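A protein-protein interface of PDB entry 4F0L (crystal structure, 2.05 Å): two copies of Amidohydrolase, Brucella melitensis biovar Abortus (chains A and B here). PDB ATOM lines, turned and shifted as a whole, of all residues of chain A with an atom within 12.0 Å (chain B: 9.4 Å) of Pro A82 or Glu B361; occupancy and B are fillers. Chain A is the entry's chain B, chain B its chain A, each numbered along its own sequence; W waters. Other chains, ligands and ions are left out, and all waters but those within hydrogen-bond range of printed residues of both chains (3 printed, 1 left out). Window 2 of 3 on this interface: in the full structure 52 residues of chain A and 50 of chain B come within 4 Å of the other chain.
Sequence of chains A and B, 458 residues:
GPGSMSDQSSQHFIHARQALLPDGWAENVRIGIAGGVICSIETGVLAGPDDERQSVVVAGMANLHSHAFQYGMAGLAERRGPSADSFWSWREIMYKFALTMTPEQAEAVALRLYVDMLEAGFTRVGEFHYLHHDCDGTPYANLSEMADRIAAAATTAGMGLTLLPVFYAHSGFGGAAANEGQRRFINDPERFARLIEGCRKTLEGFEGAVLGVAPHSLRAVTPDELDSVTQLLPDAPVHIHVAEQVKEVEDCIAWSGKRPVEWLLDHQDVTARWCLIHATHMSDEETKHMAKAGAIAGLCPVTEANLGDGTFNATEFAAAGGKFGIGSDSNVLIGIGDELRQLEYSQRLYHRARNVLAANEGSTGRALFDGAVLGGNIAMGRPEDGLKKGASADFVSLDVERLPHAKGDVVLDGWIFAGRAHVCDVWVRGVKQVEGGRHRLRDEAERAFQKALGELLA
The backbone NH (N) of Gly A81 sits at hydrogen-bond distance from the backbone carbonyl oxygen (O) of Glu B361.
The guanidinium group (NH1) of Arg A79 lies within salt-bridge range of the side-chain carboxylate (OD2) of Asp B409.
ND2 of Asn B355 lies within hydrogen-bond range of O of Ala A77 (3.3 Å).
The backbone NH (N) of Thr B364 sits at hydrogen-bond distance from the backbone carbonyl oxygen (O) of Glu A78, at 2.8 Å.
OD1 of Asn B355 sits close to O of Glu A78 (3.0 Å).
ND2 of Asn B355 sits at hydrogen-bond distance from O of Arg A79, 3.5 Å away.
N of Arg A80 is in hydrogen-bond range of O of Gly B362.
The guanidinium group (NH1) of Arg A80 is in hydrogen-bond range of the backbone carbonyl oxygen (O) of Ser A83, at 2.6 Å.
OD1 of Asp B409 is in salt-bridge range of NH1 of Arg B366, 3.0 Å away.
The backbone carbonyl oxygen (O) of Arg A79 sits at hydrogen-bond distance from the side-chain hydroxyl (OG) of Ser A89 (3.2 Å).
N of Arg B366 is in hydrogen-bond range of OG of Ser B363 (3.0 Å).
The side-chain hydroxyl (OG) of Ser B363 lies within hydrogen-bond range of the side-chain carboxylate (OD2) of Asp B413 (2.8 Å).
The side-chain hydroxyl (OG1) of Thr B364 lies within hydrogen-bond range of the side-chain amide oxygen (OD1) of Asn B355 (2.7 Å).
Among the printed residues, pairs that only touch across the chains: Gly A75 with Asp B413 (3.4 Å), Arg A79 with Gly B362 (3.4 Å), Arg A80 with Asn B355 (3.5 Å), Arg A79 with Ser B363 (3.5 Å), Pro A82 with Glu B361 (3.5 Å), Arg A80 with Ala B358 (3.6 Å), Arg A80 with Glu B361 (3.7 Å), Glu A78 with Ser B363 (3.7 Å), Ser A89 with Asn B355 (3.7 Å) and Glu A78 with Asp B413 (3.8 Å).
Of the printed residues of chain B, Gly A75 touches Asp B413.
Printed residues of chain B within 4 Å of Ala A77: Asn B355 (3.3 Å).
Printed residues of chain B within 4 Å of Glu A78: Asn B355, Ser B363, Thr B364 and Asp B413.
Printed residues of chain B within 4 Å of Arg A79: Asn B355 (3.5 Å), Gly B362 (3.4 Å), Ser B363 (3.5 Å) and Asp B409 (3.0 Å).
Of the printed residues of chain B, Arg A80 touches Asn B355, Ala B358, Glu B361 and Gly B362.
Pro A82 touches one residue of chain B.
Phe A87 touches none of the printed residues of chain B.
Glu A92 touches none of the printed residues of chain B.
Ala B358 touches one residue of chain A.
No residue of chain A comes within 4 Å of Ala B359.
Glu B361 touches just these residues of chain A: Arg A80 (3.7 Å), Gly A81 (3.1 Å) and Pro A82 (3.5 Å).
Of the printed residues of chain A, Gly B362 touches Arg A79 (3.4 Å) and Arg A80 (2.9 Å).
The nearest residue of chain A that does not touch Glu B361 is Arg A79 (4.4 Å).
The nearest printed residue of chain B that does not touch Ser A89 is Glu B361 (7.8 Å).
Of the 13 printed residues of chain B, 8 touch a printed residue of chain A.
Of the 19 printed residues of chain A, 8 touch a printed residue of chain B.
Hydrophobic or aromatic side chains of chain A within 4 Å of the printed part of chain B: Pro A82.
Among the printed residues, 17 pairs touch across the chains.
Among the printed residues, Asp or Glu carboxylates within 4 Å of a Lys or Arg side-chain nitrogen of the other chain: Arg A79 with Asp B409 (3.0 Å).
No position is printed for both chains.
Of the 17 pairs that touch across the chains among the printed residues, none has its exchanged pair printed and touching as well.
Water W3 lies within hydrogen-bond range of the side-chain carboxylate (OD2) of Asp B409 (2.5 Å), the backbone NH (N) of Ser B363 (3.0 Å) and the guanidinium group (NH2) of Arg A79 (3.5 Å).
Water W2 lies within hydrogen-bond range of OD2 of Asp B413 (2.6 Å) and NH1 of Arg A79 (3.5 Å).
Water W1 lies within hydrogen-bond range of O of Ser A86 (2.7 Å), O of Arg A80 (3.0 Å), ND2 of Asn B355 (3.0 Å) and OG of Ser A89 (3.2 Å).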
ATOM      1  N   GLY A  75     -22.910 -28.563  12.586  1.00  0.00           N
ATOM      2  CA  GLY A  75     -21.483 -28.675  12.324  1.00  0.00           C
ATOM      3  C   GLY A  75     -21.135 -29.572  11.149  1.00  0.00           C
ATOM      4  O   GLY A  75     -19.989 -29.610  10.745  1.00  0.00           O
ATOM      5  N   LEU A  76     -22.126 -30.257  10.586  1.00  0.00           N
ATOM      6  CA  LEU A  76     -21.948 -31.151   9.485  1.00  0.00           C
ATOM      7  C   LEU A  76     -22.283 -30.527   8.116  1.00  0.00           C
ATOM      8  O   LEU A  76     -21.986 -31.139   7.127  1.00  0.00           O
ATOM      9  CB  LEU A  76     -22.753 -32.454   9.714  1.00  0.00           C
ATOM     10  CG  LEU A  76     -22.482 -33.227  11.046  1.00  0.00           C
ATOM     11  CD1 LEU A  76     -23.303 -34.513  11.150  1.00  0.00           C
ATOM     12  CD2 LEU A  76     -21.021 -33.600  11.257  1.00  0.00           C
ATOM     13  N   ALA A  77     -22.859 -29.320   8.058  1.00  0.00           N
ATOM     14  CA  ALA A  77     -23.226 -28.698   6.769  1.00  0.00           C
ATOM     15  C   ALA A  77     -22.249 -27.592   6.315  1.00  0.00           C
ATOM     16  O   ALA A  77     -22.650 -26.676   5.585  1.00  0.00           O
ATOM     17  CB  ALA A  77     -24.652 -28.146   6.829  1.00  0.00           C
ATOM     18  N   GLU A  78     -20.986 -27.668   6.741  1.00  0.00           N
ATOM     19  CA  GLU A  78     -20.028 -26.601   6.477  1.00  0.00           C
ATOM     20  C   GLU A  78     -18.949 -27.005   5.453  1.00  0.00           C
ATOM     21  O   GLU A  78     -17.853 -26.444   5.461  1.00  0.00           O
ATOM     22  CB  GLU A  78     -19.374 -26.104   7.766  1.00  0.00           C
ATOM     23  CG  GLU A  78     -20.354 -25.861   8.927  1.00  0.00           C
ATOM     24  CD  GLU A  78     -21.494 -24.896   8.623  1.00  0.00           C
ATOM     25  OE1 GLU A  78     -21.301 -23.945   7.826  1.00  0.00           O
ATOM     26  OE2 GLU A  78     -22.601 -25.089   9.185  1.00  0.00           O
ATOM     27  N   ARG A  79     -19.278 -27.962   4.589  1.00  0.00           N
ATOM     28  CA  ARG A  79     -18.415 -28.365   3.485  1.00  0.00           C
ATOM     29  C   ARG A  79     -19.032 -27.913   2.182  1.00  0.00           C
ATOM     30  O   ARG A  79     -20.215 -28.146   1.946  1.00  0.00           O
ATOM     31  CB  ARG A  79     -18.254 -29.876   3.430  1.00  0.00           C
ATOM     32  CG  ARG A  79     -17.459 -30.482   4.570  1.00  0.00           C
ATOM     33  CD  ARG A  79     -17.132 -31.938   4.284  1.00  0.00           C
ATOM     34  NE  ARG A  79     -16.051 -32.111   3.315  1.00  0.00           N
ATOM     35  CZ  ARG A  79     -14.738 -32.088   3.592  1.00  0.00           C
ATOM     36  NH1 ARG A  79     -14.286 -31.889   4.831  1.00  0.00           N
ATOM     37  NH2 ARG A  79     -13.862 -32.268   2.612  1.00  0.00           N
ATOM     38  N   ARG A  80     -18.240 -27.266   1.339  1.00  0.00           N
ATOM     39  CA  ARG A  80     -18.783 -26.582   0.150  1.00  0.00           C
ATOM     40  C   ARG A  80     -19.397 -27.558  -0.854  1.00  0.00           C
ATOM     41  O   ARG A  80     -20.474 -27.299  -1.377  1.00  0.00           O
ATOM     42  CB  ARG A  80     -17.708 -25.708  -0.528  1.00  0.00           C
ATOM     43  CG  ARG A  80     -18.124 -25.045  -1.845  1.00  0.00           C
ATOM     44  CD  ARG A  80     -19.227 -23.995  -1.646  1.00  0.00           C
ATOM     45  NE  ARG A  80     -19.657 -23.429  -2.934  1.00  0.00           N
ATOM     46  CZ  ARG A  80     -20.451 -24.040  -3.826  1.00  0.00           C
ATOM     47  NH1 ARG A  80     -20.964 -25.252  -3.585  1.00  0.00           N
ATOM     48  NH2 ARG A  80     -20.756 -23.427  -4.964  1.00  0.00           N
ATOM     49  N   GLY A  81     -18.694 -28.647  -1.153  1.00  0.00           N
ATOM     50  CA  GLY A  81     -19.165 -29.631  -2.134  1.00  0.00           C
ATOM     51  C   GLY A  81     -19.030 -29.155  -3.581  1.00  0.00           C
ATOM     52  O   GLY A  81     -18.665 -28.015  -3.836  1.00  0.00           O
ATOM     53  N   PRO A  82     -19.335 -30.034  -4.552  1.00  0.00           N
ATOM     54  CA  PRO A  82     -19.152 -29.667  -5.969  1.00  0.00           C
ATOM     55  C   PRO A  82     -20.267 -28.829  -6.642  1.00  0.00           C
ATOM     56  O   PRO A  82     -20.076 -28.413  -7.788  1.00  0.00           O
ATOM     57  CB  PRO A  82     -19.016 -31.036  -6.670  1.00  0.00           C
ATOM     58  CG  PRO A  82     -19.790 -31.992  -5.800  1.00  0.00           C
ATOM     59  CD  PRO A  82     -19.741 -31.447  -4.383  1.00  0.00           C
ATOM     60  N   SER A  83     -21.405 -28.585  -5.984  1.00  0.00           N
ATOM     61  CA  SER A  83     -22.537 -27.911  -6.655  1.00  0.00           C
ATOM     62  C   SER A  83     -22.324 -26.415  -6.877  1.00  0.00           C
ATOM     63  O   SER A  83     -21.755 -25.731  -6.018  1.00  0.00           O
ATOM     64  CB  SER A  83     -23.833 -28.093  -5.850  1.00  0.00           C
ATOM     65  OG  SER A  83     -24.932 -27.473  -6.501  1.00  0.00           O
ATOM     66  N   ALA A  84     -22.831 -25.906  -8.004  1.00  0.00           N
ATOM     67  CA  ALA A  84     -22.897 -24.451  -8.279  1.00  0.00           C
ATOM     68  C   ALA A  84     -23.803 -23.746  -7.278  1.00  0.00           C
ATOM     69  O   ALA A  84     -23.615 -22.563  -6.974  1.00  0.00           O
ATOM     70  CB  ALA A  84     -23.414 -24.189  -9.702  1.00  0.00           C
ATOM     71  N   ASP A  85     -24.798 -24.486  -6.787  1.00  0.00           N
ATOM     72  CA  ASP A  85     -25.698 -24.003  -5.750  1.00  0.00           C
ATOM     73  C   ASP A  85     -25.028 -24.206  -4.357  1.00  0.00           C
ATOM     74  O   ASP A  85     -24.959 -25.326  -3.859  1.00  0.00           O
ATOM     75  CB  ASP A  85     -27.048 -24.740  -5.850  1.00  0.00           C
ATOM     76  CG  ASP A  85     -28.062 -24.279  -4.806  1.00  0.00           C
ATOM     77  OD1 ASP A  85     -27.788 -23.333  -4.024  1.00  0.00           O
ATOM     78  OD2 ASP A  85     -29.150 -24.876  -4.765  1.00  0.00           O
ATOM     79  N   SER A  86     -24.538 -23.116  -3.748  1.00  0.00           N
ATOM     80  CA  SER A  86     -23.870 -23.191  -2.426  1.00  0.00           C
ATOM     81  C   SER A  86     -24.789 -23.629  -1.267  1.00  0.00           C
ATOM     82  O   SER A  86     -24.295 -23.897  -0.161  1.00  0.00           O
ATOM     83  CB  SER A  86     -23.170 -21.863  -2.077  1.00  0.00           C
ATOM     84  OG  SER A  86     -24.076 -20.889  -1.601  1.00  0.00           O
ATOM     85  N   PHE A  87     -26.103 -23.719  -1.504  1.00  0.00           N
ATOM     86  CA  PHE A  87     -27.040 -24.271  -0.496  1.00  0.00           C
ATOM     87  C   PHE A  87     -27.313 -25.781  -0.631  1.00  0.00           C
ATOM     88  O   PHE A  87     -28.025 -26.346   0.198  1.00  0.00           O
ATOM     89  CB  PHE A  87     -28.368 -23.504  -0.545  1.00  0.00           C
ATOM     90  CG  PHE A  87     -28.203 -22.045  -0.275  1.00  0.00           C
ATOM     91  CD1 PHE A  87     -28.246 -21.566   1.019  1.00  0.00           C
ATOM     92  CD2 PHE A  87     -27.955 -21.154  -1.311  1.00  0.00           C
ATOM     93  CE1 PHE A  87     -28.063 -20.223   1.283  1.00  0.00           C
ATOM     94  CE2 PHE A  87     -27.789 -19.802  -1.052  1.00  0.00           C
ATOM     95  CZ  PHE A  87     -27.839 -19.337   0.258  1.00  0.00           C
ATOM     96  N   TRP A  88     -26.770 -26.417  -1.667  1.00  0.00           N
ATOM     97  CA  TRP A  88     -27.068 -27.835  -1.958  1.00  0.00           C
ATOM     98  C   TRP A  88     -26.661 -28.730  -0.806  1.00  0.00           C
ATOM     99  O   TRP A  88     -27.456 -29.563  -0.350  1.00  0.00           O
ATOM    100  CB  TRP A  88     -26.402 -28.308  -3.258  1.00  0.00           C
ATOM    101  N   SER A  89     -25.440 -28.534  -0.299  1.00  0.00           N
ATOM    102  CA  SER A  89     -24.918 -29.377   0.792  1.00  0.00           C
ATOM    103  C   SER A  89     -25.802 -29.327   2.054  1.00  0.00           C
ATOM    104  O   SER A  89     -26.020 -30.360   2.702  1.00  0.00           O
ATOM    105  CB  SER A  89     -23.464 -29.013   1.111  1.00  0.00           C
ATOM    106  OG  SER A  89     -23.342 -27.670   1.580  1.00  0.00           O
ATOM    107  N   TRP A  90     -26.320 -28.144   2.385  1.00  0.00           N
ATOM    108  CA  TRP A  90     -27.212 -27.997   3.538  1.00  0.00           C
ATOM    109  C   TRP A  90     -28.485 -28.796   3.350  1.00  0.00           C
ATOM    110  O   TRP A  90     -28.881 -29.551   4.219  1.00  0.00           O
ATOM    111  CB  TRP A  90     -27.561 -26.529   3.788  1.00  0.00           C
ATOM    112  CG  TRP A  90     -28.245 -26.320   5.106  1.00  0.00           C
ATOM    113  CD1 TRP A  90     -27.655 -26.005   6.327  1.00  0.00           C
ATOM    114  CD2 TRP A  90     -29.689 -26.401   5.385  1.00  0.00           C
ATOM    115  NE1 TRP A  90     -28.606 -25.886   7.310  1.00  0.00           N
ATOM    116  CE2 TRP A  90     -29.845 -26.123   6.819  1.00  0.00           C
ATOM    117  CE3 TRP A  90     -30.816 -26.667   4.622  1.00  0.00           C
ATOM    118  CZ2 TRP A  90     -31.085 -26.119   7.439  1.00  0.00           C
ATOM    119  CZ3 TRP A  90     -32.059 -26.678   5.255  1.00  0.00           C
ATOM    120  CH2 TRP A  90     -32.192 -26.391   6.632  1.00  0.00           C
ATOM    121  N   ARG A  91     -29.132 -28.635   2.211  1.00  0.00           N
ATOM    122  CA  ARG A  91     -30.336 -29.418   1.911  1.00  0.00           C
ATOM    123  C   ARG A  91     -30.072 -30.933   1.856  1.00  0.00           C
ATOM    124  O   ARG A  91     -30.890 -31.707   2.338  1.00  0.00           O
ATOM    125  CB  ARG A  91     -30.985 -28.941   0.605  1.00  0.00           C
ATOM    126  CG  ARG A  91     -31.529 -27.520   0.689  1.00  0.00           C
ATOM    127  CD  ARG A  91     -32.668 -27.286  -0.292  1.00  0.00           C
ATOM    128  NE  ARG A  91     -32.309 -27.751  -1.629  1.00  0.00           N
ATOM    129  CZ  ARG A  91     -31.481 -27.115  -2.461  1.00  0.00           C
ATOM    130  NH1 ARG A  91     -30.889 -25.971  -2.122  1.00  0.00           N
ATOM    131  NH2 ARG A  91     -31.239 -27.639  -3.659  1.00  0.00           N
ATOM    132  N   GLU A  92     -28.941 -31.346   1.282  1.00  0.00           N
ATOM    133  CA  GLU A  92     -28.604 -32.783   1.200  1.00  0.00           C
ATOM    134  C   GLU A  92     -28.480 -33.386   2.604  1.00  0.00           C
ATOM    135  O   GLU A  92     -29.047 -34.448   2.874  1.00  0.00           O
ATOM    136  CB  GLU A  92     -27.319 -33.055   0.396  1.00  0.00           C
ATOM    137  CG  GLU A  92     -26.834 -34.506   0.515  1.00  0.00           C
ATOM    138  CD  GLU A  92     -25.855 -34.939  -0.576  1.00  0.00           C
ATOM    139  OE1 GLU A  92     -24.920 -34.169  -0.896  1.00  0.00           O
ATOM    140  OE2 GLU A  92     -26.012 -36.074  -1.105  1.00  0.00           O
ATOM    141  N   ILE A  93     -27.733 -32.711   3.482  1.00  0.00           N
ATOM    142  CA  ILE A  93     -27.543 -33.196   4.838  1.00  0.00           C
ATOM    143  C   ILE A  93     -28.890 -33.131   5.571  1.00  0.00           C
ATOM    144  O   ILE A  93     -29.270 -34.087   6.231  1.00  0.00           O
ATOM    145  CB  ILE A  93     -26.445 -32.437   5.601  1.00  0.00           C
ATOM    146  CG1 ILE A  93     -25.080 -32.536   4.876  1.00  0.00           C
ATOM    147  CG2 ILE A  93     -26.320 -32.975   7.020  1.00  0.00           C
ATOM    148  CD1 ILE A  93     -24.599 -33.944   4.548  1.00  0.00           C
ATOM    149  N   ASN B 355     -20.670 -21.512   2.829  1.00  0.00           N
ATOM    150  CA  ASN B 355     -19.312 -22.050   2.624  1.00  0.00           C
ATOM    151  C   ASN B 355     -18.534 -21.207   1.603  1.00  0.00           C
ATOM    152  O   ASN B 355     -17.974 -21.717   0.623  1.00  0.00           O
ATOM    153  CB  ASN B 355     -19.440 -23.527   2.248  1.00  0.00           C
ATOM    154  CG  ASN B 355     -20.105 -24.318   3.368  1.00  0.00           C
ATOM    155  OD1 ASN B 355     -19.653 -24.225   4.516  1.00  0.00           O
ATOM    156  ND2 ASN B 355     -21.208 -25.028   3.067  1.00  0.00           N
ATOM    157  N   LEU B 357     -15.805 -19.205   2.143  1.00  0.00           N
ATOM    158  CA  LEU B 357     -14.335 -19.254   2.271  1.00  0.00           C
ATOM    159  C   LEU B 357     -13.727 -20.672   2.295  1.00  0.00           C
ATOM    160  O   LEU B 357     -12.525 -20.831   2.523  1.00  0.00           O
ATOM    161  CB  LEU B 357     -13.887 -18.402   3.468  1.00  0.00           C
ATOM    162  CG  LEU B 357     -14.398 -16.943   3.354  1.00  0.00           C
ATOM    163  CD1 LEU B 357     -13.868 -16.022   4.460  1.00  0.00           C
ATOM    164  CD2 LEU B 357     -14.100 -16.391   1.976  1.00  0.00           C
ATOM    165  N   ALA B 358     -14.537 -21.695   2.031  1.00  0.00           N
ATOM    166  CA  ALA B 358     -13.997 -23.030   1.708  1.00  0.00           C
ATOM    167  C   ALA B 358     -13.014 -22.957   0.512  1.00  0.00           C
ATOM    168  O   ALA B 358     -13.149 -22.101  -0.359  1.00  0.00           O
ATOM    169  CB  ALA B 358     -15.125 -24.005   1.361  1.00  0.00           C
ATOM    170  N   ALA B 359     -12.061 -23.886   0.486  1.00  0.00           N
ATOM    171  CA  ALA B 359     -11.088 -24.011  -0.592  1.00  0.00           C
ATOM    172  C   ALA B 359     -11.393 -25.307  -1.356  1.00  0.00           C
ATOM    173  O   ALA B 359     -11.517 -26.381  -0.757  1.00  0.00           O
ATOM    174  CB  ALA B 359      -9.674 -24.026  -0.018  1.00  0.00           C
ATOM    175  N   ASN B 360     -11.536 -25.200  -2.673  1.00  0.00           N
ATOM    176  CA  ASN B 360     -11.957 -26.333  -3.507  1.00  0.00           C
ATOM    177  C   ASN B 360     -13.392 -26.714  -3.072  1.00  0.00           C
ATOM    178  O   ASN B 360     -14.236 -25.816  -2.890  1.00  0.00           O
ATOM    179  CB  ASN B 360     -10.952 -27.494  -3.413  1.00  0.00           C
ATOM    180  N   GLU B 361     -13.690 -27.997  -2.879  1.00  0.00           N
ATOM    181  CA  GLU B 361     -15.001 -28.347  -2.320  1.00  0.00           C
ATOM    182  C   GLU B 361     -14.933 -28.761  -0.850  1.00  0.00           C
ATOM    183  O   GLU B 361     -15.806 -29.459  -0.353  1.00  0.00           O
ATOM    184  CB  GLU B 361     -15.670 -29.420  -3.133  1.00  0.00           C
ATOM    185  CG  GLU B 361     -14.866 -30.680  -3.356  1.00  0.00           C
ATOM    186  CD  GLU B 361     -15.362 -31.407  -4.593  1.00  0.00           C
ATOM    187  OE1 GLU B 361     -15.488 -32.643  -4.529  1.00  0.00           O
ATOM    188  OE2 GLU B 361     -15.641 -30.732  -5.616  1.00  0.00           O
ATOM    189  N   GLY B 362     -13.924 -28.258  -0.152  1.00  0.00           N
ATOM    190  CA  GLY B 362     -13.614 -28.714   1.195  1.00  0.00           C
ATOM    191  C   GLY B 362     -14.423 -28.111   2.321  1.00  0.00           C
ATOM    192  O   GLY B 362     -15.461 -27.460   2.116  1.00  0.00           O
ATOM    193  N   SER B 363     -13.940 -28.380   3.526  1.00  0.00           N
ATOM    194  CA  SER B 363     -14.501 -27.856   4.768  1.00  0.00           C
ATOM    195  C   SER B 363     -14.173 -26.355   4.886  1.00  0.00           C
ATOM    196  O   SER B 363     -13.046 -25.942   4.628  1.00  0.00           O
ATOM    197  CB  SER B 363     -13.919 -28.630   5.958  1.00  0.00           C
ATOM    198  OG  SER B 363     -14.000 -27.901   7.170  1.00  0.00           O
ATOM    199  N   THR B 364     -15.162 -25.555   5.261  1.00  0.00           N
ATOM    200  CA  THR B 364     -14.932 -24.133   5.475  1.00  0.00           C
ATOM    201  C   THR B 364     -14.037 -23.963   6.702  1.00  0.00           C
ATOM    202  O   THR B 364     -13.134 -23.134   6.711  1.00  0.00           O
ATOM    203  CB  THR B 364     -16.281 -23.370   5.650  1.00  0.00           C
ATOM    204  OG1 THR B 364     -17.044 -23.493   4.442  1.00  0.00           O
ATOM    205  CG2 THR B 364     -16.075 -21.894   5.996  1.00  0.00           C
ATOM    206  N   ARG B 366     -11.817 -26.017   7.958  1.00  0.00           N
ATOM    207  CA  ARG B 366     -10.467 -26.422   7.540  1.00  0.00           C
ATOM    208  C   ARG B 366      -9.732 -25.302   6.816  1.00  0.00           C
ATOM    209  O   ARG B 366      -8.580 -24.960   7.155  1.00  0.00           O
ATOM    210  CB  ARG B 366     -10.549 -27.697   6.705  1.00  0.00           C
ATOM    211  CG  ARG B 366      -9.276 -28.159   5.987  1.00  0.00           C
ATOM    212  CD  ARG B 366      -8.160 -28.560   6.943  1.00  0.00           C
ATOM    213  NE  ARG B 366      -6.994 -28.964   6.138  1.00  0.00           N
ATOM    214  CZ  ARG B 366      -6.907 -30.115   5.477  1.00  0.00           C
ATOM    215  NH1 ARG B 366      -7.896 -30.992   5.549  1.00  0.00           N
ATOM    216  NH2 ARG B 366      -5.823 -30.407   4.743  1.00  0.00           N
ATOM    217  N   ALA B 367     -10.359 -24.753   5.789  1.00  0.00           N
ATOM    218  CA  ALA B 367      -9.720 -23.729   4.995  1.00  0.00           C
ATOM    219  C   ALA B 367      -9.383 -22.508   5.844  1.00  0.00           C
ATOM    220  O   ALA B 367      -8.315 -21.933   5.718  1.00  0.00           O
ATOM    221  CB  ALA B 367     -10.634 -23.323   3.826  1.00  0.00           C
ATOM    222  N   ASP B 409     -11.461 -32.819   9.760  1.00  0.00           N
ATOM    223  CA  ASP B 409     -12.189 -31.649   9.286  1.00  0.00           C
ATOM    224  C   ASP B 409     -13.517 -31.457  10.048  1.00  0.00           C
ATOM    225  O   ASP B 409     -13.896 -30.323  10.399  1.00  0.00           O
ATOM    226  CB  ASP B 409     -12.473 -31.690   7.779  1.00  0.00           C
ATOM    227  CG  ASP B 409     -11.259 -31.428   6.937  1.00  0.00           C
ATOM    228  OD1 ASP B 409     -10.164 -31.104   7.450  1.00  0.00           O
ATOM    229  OD2 ASP B 409     -11.423 -31.524   5.709  1.00  0.00           O
ATOM    230  N   ASP B 413     -14.893 -28.114  12.011  1.00  0.00           N
ATOM    231  CA  ASP B 413     -16.206 -27.496  11.784  1.00  0.00           C
ATOM    232  C   ASP B 413     -17.036 -27.504  13.065  1.00  0.00           C
ATOM    233  O   ASP B 413     -17.794 -26.579  13.328  1.00  0.00           O
ATOM    234  CB  ASP B 413     -16.940 -28.173  10.608  1.00  0.00           C
ATOM    235  CG  ASP B 413     -16.336 -27.830   9.263  1.00  0.00           C
ATOM    236  OD1 ASP B 413     -15.753 -26.739   9.137  1.00  0.00           O
ATOM    237  OD2 ASP B 413     -16.416 -28.638   8.324  1.00  0.00           O
HETATM  238  O   HOH W   1     -21.919 -25.168   0.155  1.00  0.00           O
HETATM  239  O   HOH W   2     -16.141 -31.143   7.703  1.00  0.00           O
HETATM  240  O   HOH W   3     -11.427 -30.047   3.635  1.00  0.00           O
